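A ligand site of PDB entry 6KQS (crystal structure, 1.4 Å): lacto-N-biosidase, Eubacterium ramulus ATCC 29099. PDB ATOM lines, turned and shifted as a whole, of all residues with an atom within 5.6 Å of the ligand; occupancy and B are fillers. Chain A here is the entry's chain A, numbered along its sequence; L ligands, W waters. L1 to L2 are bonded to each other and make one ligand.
OD2 of Asp 570 sits at hydrogen-bond distance from O1 of LIG L1, at 2.5 Å.
The side-chain carboxylate (OD2) of Asp 338 sits at hydrogen-bond distance from an oxygen (O2) of LG2 L2, at 2.6 Å.
O3 of LG2 L2 is in hydrogen-bond range of NE2 of His 420 (2.7 Å).
The side-chain amino group of Lys 419 lies within hydrogen-bond range of an oxygen (O3) of LIG L1, at 2.8 Å.
N1 of LIG L1 sits at hydrogen-bond distance from OD1 of Asp 577 (2.8 Å).
NE2 of His 342 lies within hydrogen-bond range of O2 of LG2 L2.
An oxygen (O5) of LIG L1 lies close to the backbone NH of Ala 544, 3.3 Å away.
The indole nitrogen of Trp 550 sits close to an oxygen (O5) of LG2 L2 (3.3 Å).
The side-chain sulfur (SG) of Cys 600 sits close to a nitrogen (N1) of LIG L1 (3.5 Å).
The side-chain carboxylate (OD2) of Asp 575 sits close to an oxygen (O4) of LIG L1 (3.3 Å).
Tyr 466 touches the ligand.
OD1 of Asp 504 touches C6 of LIG L1, 3.6 Å away.
CB of Val 543 touches O5 of LIG L1, 3.4 Å away.
N of Ala 545 touches O5 of LIG L1 (3.7 Å).
Trp 548 touches the ligand.
Ser 578 touches the ligand.
CE of Met 598 touches O4 of LIG L1, at 3.4 Å.
CD1 of Leu 601 touches O6 of LIG L1, 3.9 Å away.
Hydrophobic or aromatic side chains that line the ligand: His 342, His 420, Tyr 466, Val 543, Trp 548, Trp 550, Met 598 and Leu 601.
Water W4 lies within hydrogen-bond range of an oxygen (O3) of LIG L1 (2.6 Å), the side-chain carboxylate of Asp 504 (2.6 Å), the backbone carbonyl oxygen of Val 543 (2.8 Å) and the guanidinium group of Arg 459 (3.1 Å).
Water W2 lies within hydrogen-bond range of O6 of LIG L1 (3.0 Å) and SG of Cys 600 (3.6 Å).
Water W8 lies within hydrogen-bond range of NZ of Lys 419 (2.8 Å) and O2 of LIG L1 (3.5 Å).
The backbone NH of Asp 570 sits at hydrogen-bond distance from the side-chain amide oxygen of Asn 568 (2.9 Å).
OD1 of Asp 338 lies within hydrogen-bond range of NE2 of His 342 (3.4 Å).
OD1 of Asp 338 sits at hydrogen-bond distance from OH of Tyr 466 (2.6 Å).
The backbone NH (N) of Asp 577 sits close to the side-chain carboxylate (OD1) of Asp 575, 3.3 Å away.
The backbone NH (N) of Ala 544 lies within hydrogen-bond range of the side-chain amide oxygen (OD1) of Asn 568, 3.1 Å away.
OH of Tyr 510 lies within hydrogen-bond range of NE1 of Trp 550, at 2.9 Å.
O of Val 543 lies within hydrogen-bond range of NH2 of Arg 459, at 3.1 Å.
The side-chain carboxylate (OD1) of Asp 504 is in hydrogen-bond range of the backbone NH (N) of Ala 545, 2.8 Å away.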
ATOM      1  N   ASP A 338      19.554 -16.103  -4.513  1.00  0.00           N
ATOM      2  CA  ASP A 338      18.375 -15.230  -4.762  1.00  0.00           C
ATOM      3  C   ASP A 338      18.749 -13.785  -4.463  1.00  0.00           C
ATOM      4  O   ASP A 338      18.124 -12.877  -5.024  1.00  0.00           O
ATOM      5  CB  ASP A 338      17.154 -15.740  -3.981  1.00  0.00           C
ATOM      6  CG  ASP A 338      17.176 -15.430  -2.518  1.00  0.00           C
ATOM      7  OD1 ASP A 338      17.721 -16.231  -1.734  1.00  0.00           O
ATOM      8  OD2 ASP A 338      16.744 -14.330  -2.164  1.00  0.00           O
ATOM      9  N   ALA A 339      19.682 -13.548  -3.562  1.00  0.00           N
ATOM     10  CA  ALA A 339      20.263 -12.251  -3.193  1.00  0.00           C
ATOM     11  C   ALA A 339      21.750 -12.363  -3.480  1.00  0.00           C
ATOM     12  O   ALA A 339      22.401 -13.334  -3.118  1.00  0.00           O
ATOM     13  CB  ALA A 339      20.075 -11.901  -1.740  1.00  0.00           C
ATOM     14  N   HIS A 342      24.352 -13.286  -0.525  1.00  0.00           N
ATOM     15  CA  HIS A 342      24.463 -14.589   0.164  1.00  0.00           C
ATOM     16  C   HIS A 342      25.765 -15.274  -0.248  1.00  0.00           C
ATOM     17  O   HIS A 342      26.019 -15.371  -1.469  1.00  0.00           O
ATOM     18  CB  HIS A 342      23.330 -15.557  -0.155  1.00  0.00           C
ATOM     19  CG  HIS A 342      21.964 -15.112   0.315  1.00  0.00           C
ATOM     20  ND1 HIS A 342      21.762 -14.598   1.551  1.00  0.00           N
ATOM     21  CD2 HIS A 342      20.762 -15.308  -0.285  1.00  0.00           C
ATOM     22  CE1 HIS A 342      20.412 -14.381   1.682  1.00  0.00           C
ATOM     23  NE2 HIS A 342      19.817 -14.828   0.567  1.00  0.00           N
ATOM     24  N   LYS A 419      23.151 -17.902   5.509  1.00  0.00           N
ATOM     25  CA  LYS A 419      21.827 -18.569   5.460  1.00  0.00           C
ATOM     26  C   LYS A 419      21.818 -19.796   4.586  1.00  0.00           C
ATOM     27  O   LYS A 419      20.952 -20.643   4.848  1.00  0.00           O
ATOM     28  CB  LYS A 419      20.755 -17.601   4.996  1.00  0.00           C
ATOM     29  CG  LYS A 419      20.457 -16.533   6.015  1.00  0.00           C
ATOM     30  CD  LYS A 419      19.372 -15.568   5.585  1.00  0.00           C
ATOM     31  CE  LYS A 419      18.004 -16.185   5.761  1.00  0.00           C
ATOM     32  NZ  LYS A 419      16.943 -15.323   5.152  1.00  0.00           N
ATOM     33  N   HIS A 420      22.626 -19.897   3.515  1.00  0.00           N
ATOM     34  CA  HIS A 420      22.398 -20.926   2.496  1.00  0.00           C
ATOM     35  C   HIS A 420      23.617 -21.778   2.202  1.00  0.00           C
ATOM     36  O   HIS A 420      23.499 -22.746   1.445  1.00  0.00           O
ATOM     37  CB  HIS A 420      21.786 -20.314   1.219  1.00  0.00           C
ATOM     38  CG  HIS A 420      20.498 -19.628   1.511  1.00  0.00           C
ATOM     39  ND1 HIS A 420      19.436 -20.310   2.107  1.00  0.00           N
ATOM     40  CD2 HIS A 420      20.130 -18.332   1.482  1.00  0.00           C
ATOM     41  CE1 HIS A 420      18.478 -19.411   2.367  1.00  0.00           C
ATOM     42  NE2 HIS A 420      18.855 -18.224   1.963  1.00  0.00           N
ATOM     43  N   ARG A 459      23.784 -21.943  11.883  1.00  0.00           N
ATOM     44  CA  ARG A 459      22.716 -20.978  12.004  1.00  0.00           C
ATOM     45  C   ARG A 459      21.360 -21.696  12.026  1.00  0.00           C
ATOM     46  O   ARG A 459      20.540 -21.460  12.907  1.00  0.00           O
ATOM     47  CB  ARG A 459      22.758 -19.918  10.909  1.00  0.00           C
ATOM     48  CG  ARG A 459      21.546 -19.040  10.904  1.00  0.00           C
ATOM     49  CD  ARG A 459      21.679 -17.939   9.885  1.00  0.00           C
ATOM     50  NE  ARG A 459      20.366 -17.345   9.683  1.00  0.00           N
ATOM     51  CZ  ARG A 459      20.128 -16.076   9.419  1.00  0.00           C
ATOM     52  NH1 ARG A 459      21.109 -15.200   9.302  1.00  0.00           N
ATOM     53  NH2 ARG A 459      18.887 -15.681   9.357  1.00  0.00           N
ATOM     54  N   TRP A 460      21.079 -22.494  11.013  1.00  0.00           N
ATOM     55  CA  TRP A 460      19.741 -23.145  10.900  1.00  0.00           C
ATOM     56  C   TRP A 460      19.612 -24.301  11.881  1.00  0.00           C
ATOM     57  O   TRP A 460      20.573 -24.921  12.315  1.00  0.00           O
ATOM     58  CB  TRP A 460      19.514 -23.673   9.480  1.00  0.00           C
ATOM     59  CG  TRP A 460      18.195 -23.195   8.929  1.00  0.00           C
ATOM     60  CD1 TRP A 460      16.923 -23.682   9.219  1.00  0.00           C
ATOM     61  CD2 TRP A 460      17.972 -22.131   8.024  1.00  0.00           C
ATOM     62  NE1 TRP A 460      15.980 -22.992   8.554  1.00  0.00           N
ATOM     63  CE2 TRP A 460      16.574 -22.000   7.822  1.00  0.00           C
ATOM     64  CE3 TRP A 460      18.784 -21.212   7.342  1.00  0.00           C
ATOM     65  CZ2 TRP A 460      15.973 -21.022   7.019  1.00  0.00           C
ATOM     66  CZ3 TRP A 460      18.218 -20.250   6.557  1.00  0.00           C
ATOM     67  CH2 TRP A 460      16.832 -20.139   6.403  1.00  0.00           C
ATOM     68  N   TYR A 466      17.230 -25.736  -0.399  1.00  0.00           N
ATOM     69  CA  TYR A 466      17.722 -24.512  -1.093  1.00  0.00           C
ATOM     70  C   TYR A 466      18.506 -24.943  -2.334  1.00  0.00           C
ATOM     71  O   TYR A 466      19.327 -25.844  -2.257  1.00  0.00           O
ATOM     72  CB  TYR A 466      18.551 -23.598  -0.176  1.00  0.00           C
ATOM     73  CG  TYR A 466      18.544 -22.203  -0.703  1.00  0.00           C
ATOM     74  CD1 TYR A 466      17.578 -21.241  -0.376  1.00  0.00           C
ATOM     75  CD2 TYR A 466      19.462 -21.879  -1.687  1.00  0.00           C
ATOM     76  CE1 TYR A 466      17.594 -19.973  -1.001  1.00  0.00           C
ATOM     77  CE2 TYR A 466      19.480 -20.653  -2.328  1.00  0.00           C
ATOM     78  CZ  TYR A 466      18.558 -19.698  -1.988  1.00  0.00           C
ATOM     79  OH  TYR A 466      18.663 -18.454  -2.606  1.00  0.00           O
ATOM     80  N   ASP A 504      16.679 -19.875  12.309  1.00  0.00           N
ATOM     81  CA  ASP A 504      15.339 -20.444  12.058  1.00  0.00           C
ATOM     82  C   ASP A 504      15.275 -21.873  12.540  1.00  0.00           C
ATOM     83  O   ASP A 504      16.253 -22.663  12.431  1.00  0.00           O
ATOM     84  CB  ASP A 504      15.015 -20.333  10.592  1.00  0.00           C
ATOM     85  CG  ASP A 504      14.841 -18.921  10.142  1.00  0.00           C
ATOM     86  OD1 ASP A 504      13.700 -18.386  10.201  1.00  0.00           O
ATOM     87  OD2 ASP A 504      15.871 -18.337   9.694  1.00  0.00           O
ATOM     88  N   MET A 509      12.268 -25.595   1.401  1.00  0.00           N
ATOM     89  CA  MET A 509      12.475 -24.677   0.302  1.00  0.00           C
ATOM     90  C   MET A 509      12.317 -25.368  -1.063  1.00  0.00           C
ATOM     91  O   MET A 509      12.746 -26.502  -1.232  1.00  0.00           O
ATOM     92  CB  MET A 509      13.894 -24.109   0.306  1.00  0.00           C
ATOM     93  CG  MET A 509      14.208 -23.426   1.611  1.00  0.00           C
ATOM     94  SD  MET A 509      15.548 -24.225   2.689  1.00  0.00           S
ATOM     95  CE  MET A 509      16.111 -22.708   3.806  1.00  0.00           C
ATOM     96  N   TYR A 510      11.634 -24.680  -1.990  1.00  0.00           N
ATOM     97  CA  TYR A 510      11.562 -25.083  -3.377  1.00  0.00           C
ATOM     98  C   TYR A 510      10.886 -26.419  -3.589  1.00  0.00           C
ATOM     99  O   TYR A 510      11.238 -27.195  -4.473  1.00  0.00           O
ATOM    100  CB  TYR A 510      12.934 -25.058  -4.060  1.00  0.00           C
ATOM    101  CG  TYR A 510      13.533 -23.685  -4.039  1.00  0.00           C
ATOM    102  CD1 TYR A 510      12.988 -22.620  -4.726  1.00  0.00           C
ATOM    103  CD2 TYR A 510      14.636 -23.394  -3.239  1.00  0.00           C
ATOM    104  CE1 TYR A 510      13.477 -21.323  -4.612  1.00  0.00           C
ATOM    105  CE2 TYR A 510      15.120 -22.114  -3.125  1.00  0.00           C
ATOM    106  CZ  TYR A 510      14.589 -21.047  -3.821  1.00  0.00           C
ATOM    107  OH  TYR A 510      15.052 -19.773  -3.678  1.00  0.00           O
ATOM    108  N   VAL A 543      17.210 -11.943  11.296  1.00  0.00           N
ATOM    109  CA  VAL A 543      15.791 -12.277  11.503  1.00  0.00           C
ATOM    110  C   VAL A 543      15.722 -13.792  11.522  1.00  0.00           C
ATOM    111  O   VAL A 543      16.460 -14.441  10.809  1.00  0.00           O
ATOM    112  CB  VAL A 543      14.824 -11.732  10.454  1.00  0.00           C
ATOM    113  CG1 VAL A 543      14.347 -10.313  10.790  1.00  0.00           C
ATOM    114  CG2 VAL A 543      15.367 -11.882   9.061  1.00  0.00           C
ATOM    115  N   ALA A 544      14.735 -14.296  12.263  1.00  0.00           N
ATOM    116  CA  ALA A 544      14.304 -15.693  12.111  1.00  0.00           C
ATOM    117  C   ALA A 544      12.909 -15.875  12.671  1.00  0.00           C
ATOM    118  O   ALA A 544      12.516 -15.171  13.586  1.00  0.00           O
ATOM    119  CB  ALA A 544      15.254 -16.644  12.768  1.00  0.00           C
ATOM    120  N   ALA A 545      12.271 -16.881  12.117  1.00  0.00           N
ATOM    121  CA  ALA A 545      10.946 -17.359  12.553  1.00  0.00           C
ATOM    122  C   ALA A 545      11.067 -18.848  12.871  1.00  0.00           C
ATOM    123  O   ALA A 545      12.154 -19.457  12.851  1.00  0.00           O
ATOM    124  CB  ALA A 545       9.957 -17.096  11.478  1.00  0.00           C
ATOM    125  N   TRP A 548       8.532 -22.933   8.845  1.00  0.00           N
ATOM    126  CA  TRP A 548       7.988 -22.172   7.729  1.00  0.00           C
ATOM    127  C   TRP A 548       8.519 -22.641   6.381  1.00  0.00           C
ATOM    128  O   TRP A 548       9.579 -23.280   6.314  1.00  0.00           O
ATOM    129  CB  TRP A 548       8.222 -20.677   7.923  1.00  0.00           C
ATOM    130  CG  TRP A 548       9.677 -20.297   8.058  1.00  0.00           C
ATOM    131  CD1 TRP A 548      10.388 -20.284   9.192  1.00  0.00           C
ATOM    132  CD2 TRP A 548      10.485 -19.679   7.044  1.00  0.00           C
ATOM    133  NE1 TRP A 548      11.651 -19.782   8.936  1.00  0.00           N
ATOM    134  CE2 TRP A 548      11.729 -19.411   7.638  1.00  0.00           C
ATOM    135  CE3 TRP A 548      10.255 -19.372   5.713  1.00  0.00           C
ATOM    136  CZ2 TRP A 548      12.747 -18.796   6.905  1.00  0.00           C
ATOM    137  CZ3 TRP A 548      11.254 -18.800   4.985  1.00  0.00           C
ATOM    138  CH2 TRP A 548      12.469 -18.481   5.598  1.00  0.00           C
ATOM    139  N   TRP A 550       9.657 -21.675   2.240  1.00  0.00           N
ATOM    140  CA  TRP A 550      10.249 -20.696   1.327  1.00  0.00           C
ATOM    141  C   TRP A 550      10.104 -21.217  -0.101  1.00  0.00           C
ATOM    142  O   TRP A 550      10.616 -22.298  -0.444  1.00  0.00           O
ATOM    143  CB  TRP A 550      11.734 -20.522   1.654  1.00  0.00           C
ATOM    144  CG  TRP A 550      12.410 -19.729   0.586  1.00  0.00           C
ATOM    145  CD1 TRP A 550      13.224 -20.227  -0.379  1.00  0.00           C
ATOM    146  CD2 TRP A 550      12.327 -18.311   0.359  1.00  0.00           C
ATOM    147  NE1 TRP A 550      13.732 -19.194  -1.142  1.00  0.00           N
ATOM    148  CE2 TRP A 550      13.194 -18.015  -0.723  1.00  0.00           C
ATOM    149  CE3 TRP A 550      11.703 -17.238   1.012  1.00  0.00           C
ATOM    150  CZ2 TRP A 550      13.332 -16.720  -1.192  1.00  0.00           C
ATOM    151  CZ3 TRP A 550      11.844 -15.956   0.547  1.00  0.00           C
ATOM    152  CH2 TRP A 550      12.636 -15.682  -0.584  1.00  0.00           C
ATOM    153  N   ASN A 568      13.230 -10.780  17.698  1.00  0.00           N
ATOM    154  CA  ASN A 568      13.890 -10.061  16.602  1.00  0.00           C
ATOM    155  C   ASN A 568      12.817  -9.401  15.779  1.00  0.00           C
ATOM    156  O   ASN A 568      11.614  -9.433  16.171  1.00  0.00           O
ATOM    157  CB  ASN A 568      14.824 -11.029  15.852  1.00  0.00           C
ATOM    158  CG  ASN A 568      14.146 -12.163  15.131  1.00  0.00           C
ATOM    159  OD1 ASN A 568      13.666 -11.989  14.008  1.00  0.00           O
ATOM    160  ND2 ASN A 568      14.116 -13.349  15.762  1.00  0.00           N
ATOM    161  N   ASP A 570      11.371 -10.429  13.266  1.00  0.00           N
ATOM    162  CA  ASP A 570      10.403 -11.509  13.024  1.00  0.00           C
ATOM    163  C   ASP A 570      10.077 -12.127  14.389  1.00  0.00           C
ATOM    164  O   ASP A 570       9.339 -11.520  15.171  1.00  0.00           O
ATOM    165  CB  ASP A 570      10.940 -12.404  11.897  1.00  0.00           C
ATOM    166  CG  ASP A 570      10.978 -11.621  10.586  1.00  0.00           C
ATOM    167  OD1 ASP A 570      10.339 -10.538  10.474  1.00  0.00           O
ATOM    168  OD2 ASP A 570      11.611 -12.140   9.632  1.00  0.00           O
ATOM    169  N   ASP A 575       5.361 -18.529   9.534  1.00  0.00           N
ATOM    170  CA  ASP A 575       5.720 -17.509   8.499  1.00  0.00           C
ATOM    171  C   ASP A 575       5.340 -17.964   7.124  1.00  0.00           C
ATOM    172  O   ASP A 575       6.061 -18.793   6.554  1.00  0.00           O
ATOM    173  CB  ASP A 575       7.202 -17.204   8.562  1.00  0.00           C
ATOM    174  CG  ASP A 575       7.688 -16.292   7.467  1.00  0.00           C
ATOM    175  OD1 ASP A 575       6.902 -15.645   6.804  1.00  0.00           O
ATOM    176  OD2 ASP A 575       8.957 -16.313   7.279  1.00  0.00           O
ATOM    177  N   ASP A 577       5.952 -17.215   4.088  1.00  0.00           N
ATOM    178  CA  ASP A 577       6.964 -16.340   3.498  1.00  0.00           C
ATOM    179  C   ASP A 577       6.732 -16.309   1.975  1.00  0.00           C
ATOM    180  O   ASP A 577       5.725 -16.786   1.498  1.00  0.00           O
ATOM    181  CB  ASP A 577       8.368 -16.819   3.900  1.00  0.00           C
ATOM    182  CG  ASP A 577       9.396 -15.691   3.974  1.00  0.00           C
ATOM    183  OD1 ASP A 577       9.720 -15.093   2.973  1.00  0.00           O
ATOM    184  OD2 ASP A 577       9.786 -15.319   5.098  1.00  0.00           O
ATOM    185  N   SER A 578       7.676 -15.769   1.218  1.00  0.00           N
ATOM    186  CA  SER A 578       7.524 -15.833  -0.238  1.00  0.00           C
ATOM    187  C   SER A 578       7.253 -17.277  -0.646  1.00  0.00           C
ATOM    188  O   SER A 578       7.983 -18.197  -0.216  1.00  0.00           O
ATOM    189  CB  SER A 578       8.759 -15.344  -0.946  1.00  0.00           C
ATOM    190  OG  SER A 578       9.101 -14.070  -0.537  1.00  0.00           O
ATOM    191  N   MET A 598       3.303 -14.511  10.508  1.00  0.00           N
ATOM    192  CA  MET A 598       3.606 -13.494   9.526  1.00  0.00           C
ATOM    193  C   MET A 598       3.223 -13.954   8.135  1.00  0.00           C
ATOM    194  O   MET A 598       3.204 -15.126   7.823  1.00  0.00           O
ATOM    195  CB  MET A 598       5.099 -13.221   9.567  1.00  0.00           C
ATOM    196  CG  MET A 598       5.579 -12.212   8.527  1.00  0.00           C
ATOM    197  SD  MET A 598       7.393 -11.542   8.821  1.00  0.00           S
ATOM    198  CE  MET A 598       8.389 -13.099   8.575  1.00  0.00           C
ATOM    199  N   CYS A 600       4.721 -12.599   4.612  1.00  0.00           N
ATOM    200  CA  CYS A 600       5.880 -11.732   4.351  1.00  0.00           C
ATOM    201  C   CYS A 600       6.016 -11.246   2.907  1.00  0.00           C
ATOM    202  O   CYS A 600       6.571 -11.965   2.063  1.00  0.00           O
ATOM    203  CB  CYS A 600       7.128 -12.432   4.790  1.00  0.00           C
ATOM    204  SG  CYS A 600       8.498 -11.256   4.829  1.00  0.00           S
ATOM    205  N   LEU A 601       5.576 -10.010   2.718  1.00  0.00           N
ATOM    206  CA  LEU A 601       5.899  -9.203   1.507  1.00  0.00           C
ATOM    207  C   LEU A 601       5.242  -9.736   0.264  1.00  0.00           C
ATOM    208  O   LEU A 601       4.362 -10.623   0.289  1.00  0.00           O
ATOM    209  CB  LEU A 601       7.416  -8.993   1.411  1.00  0.00           C
ATOM    210  CG  LEU A 601       7.943  -8.036   2.454  1.00  0.00           C
ATOM    211  CD1 LEU A 601       9.446  -8.042   2.499  1.00  0.00           C
ATOM    212  CD2 LEU A 601       7.453  -6.593   2.206  1.00  0.00           C
HETATM  213  C1  LIG L   1      11.448 -12.879   6.328  1.00  0.00           C
HETATM  214  C2  LIG L   1      12.228 -13.022   5.029  1.00  0.00           C
HETATM  215  C3  LIG L   1      13.132 -14.259   5.018  1.00  0.00           C
HETATM  216  C4  LIG L   1      13.555 -14.583   6.434  1.00  0.00           C
HETATM  217  C5  LIG L   1      12.292 -14.998   7.190  1.00  0.00           C
HETATM  218  C6  LIG L   1      12.471 -15.428   8.601  1.00  0.00           C
HETATM  219  C7  LIG L   1      11.432 -11.867   3.055  1.00  0.00           C
HETATM  220  C8  LIG L   1      10.584 -11.962   1.859  1.00  0.00           C
HETATM  221  N1  LIG L   1      11.405 -12.975   3.825  1.00  0.00           N
HETATM  222  O1  LIG L   1      12.074 -11.861   7.181  1.00  0.00           O
HETATM  223  O2  LIG L   1      14.307 -13.867   4.272  1.00  0.00           O
HETATM  224  O3  LIG L   1      14.445 -15.701   6.393  1.00  0.00           O
HETATM  225  O4  LIG L   1      11.342 -13.977   7.194  1.00  0.00           O
HETATM  226  O5  LIG L   1      13.052 -14.457   9.416  1.00  0.00           O
HETATM  227  O6  LIG L   1      12.049 -10.856   3.402  1.00  0.00           O
HETATM  228  C1  LG2 L   2      14.374 -14.584   3.064  1.00  0.00           C
HETATM  229  C2  LG2 L   2      15.461 -13.850   2.213  1.00  0.00           C
HETATM  230  C3  LG2 L   2      15.890 -14.650   1.053  1.00  0.00           C
HETATM  231  C4  LG2 L   2      16.288 -16.041   1.472  1.00  0.00           C
HETATM  232  C5  LG2 L   2      15.064 -16.671   2.157  1.00  0.00           C
HETATM  233  C6  LG2 L   2      15.249 -18.068   2.705  1.00  0.00           C
HETATM  234  O1  LG2 L   2      14.900 -12.563   1.788  1.00  0.00           O
HETATM  235  O2  LG2 L   2      16.986 -13.960   0.393  1.00  0.00           O
HETATM  236  O3  LG2 L   2      17.409 -15.976   2.374  1.00  0.00           O
HETATM  237  O4  LG2 L   2      14.748 -15.945   3.341  1.00  0.00           O
HETATM  238  O5  LG2 L   2      15.501 -19.010   1.584  1.00  0.00           O
HETATM  239  O   HOH W   1      12.852  -9.182   1.382  1.00  0.00           O
HETATM  240  O   HOH W   2      11.321  -9.167   5.763  1.00  0.00           O
HETATM  241  O   HOH W   3      13.724  -9.577   6.286  1.00  0.00           O
HETATM  242  O   HOH W   4      15.851 -15.941   8.574  1.00  0.00           O
HETATM  243  O   HOH W   5      15.626  -9.187   1.804  1.00  0.00           O
HETATM  244  O   HOH W   6      15.434 -10.868   4.063  1.00  0.00           O
HETATM  245  O   HOH W   7      13.628 -12.063  -0.673  1.00  0.00           O
HETATM  246  O   HOH W   8      17.420 -12.549   5.173  1.00  0.00           O
HETATM  247  O   HOH W   9      17.173 -11.129   0.357  1.00  0.00           O
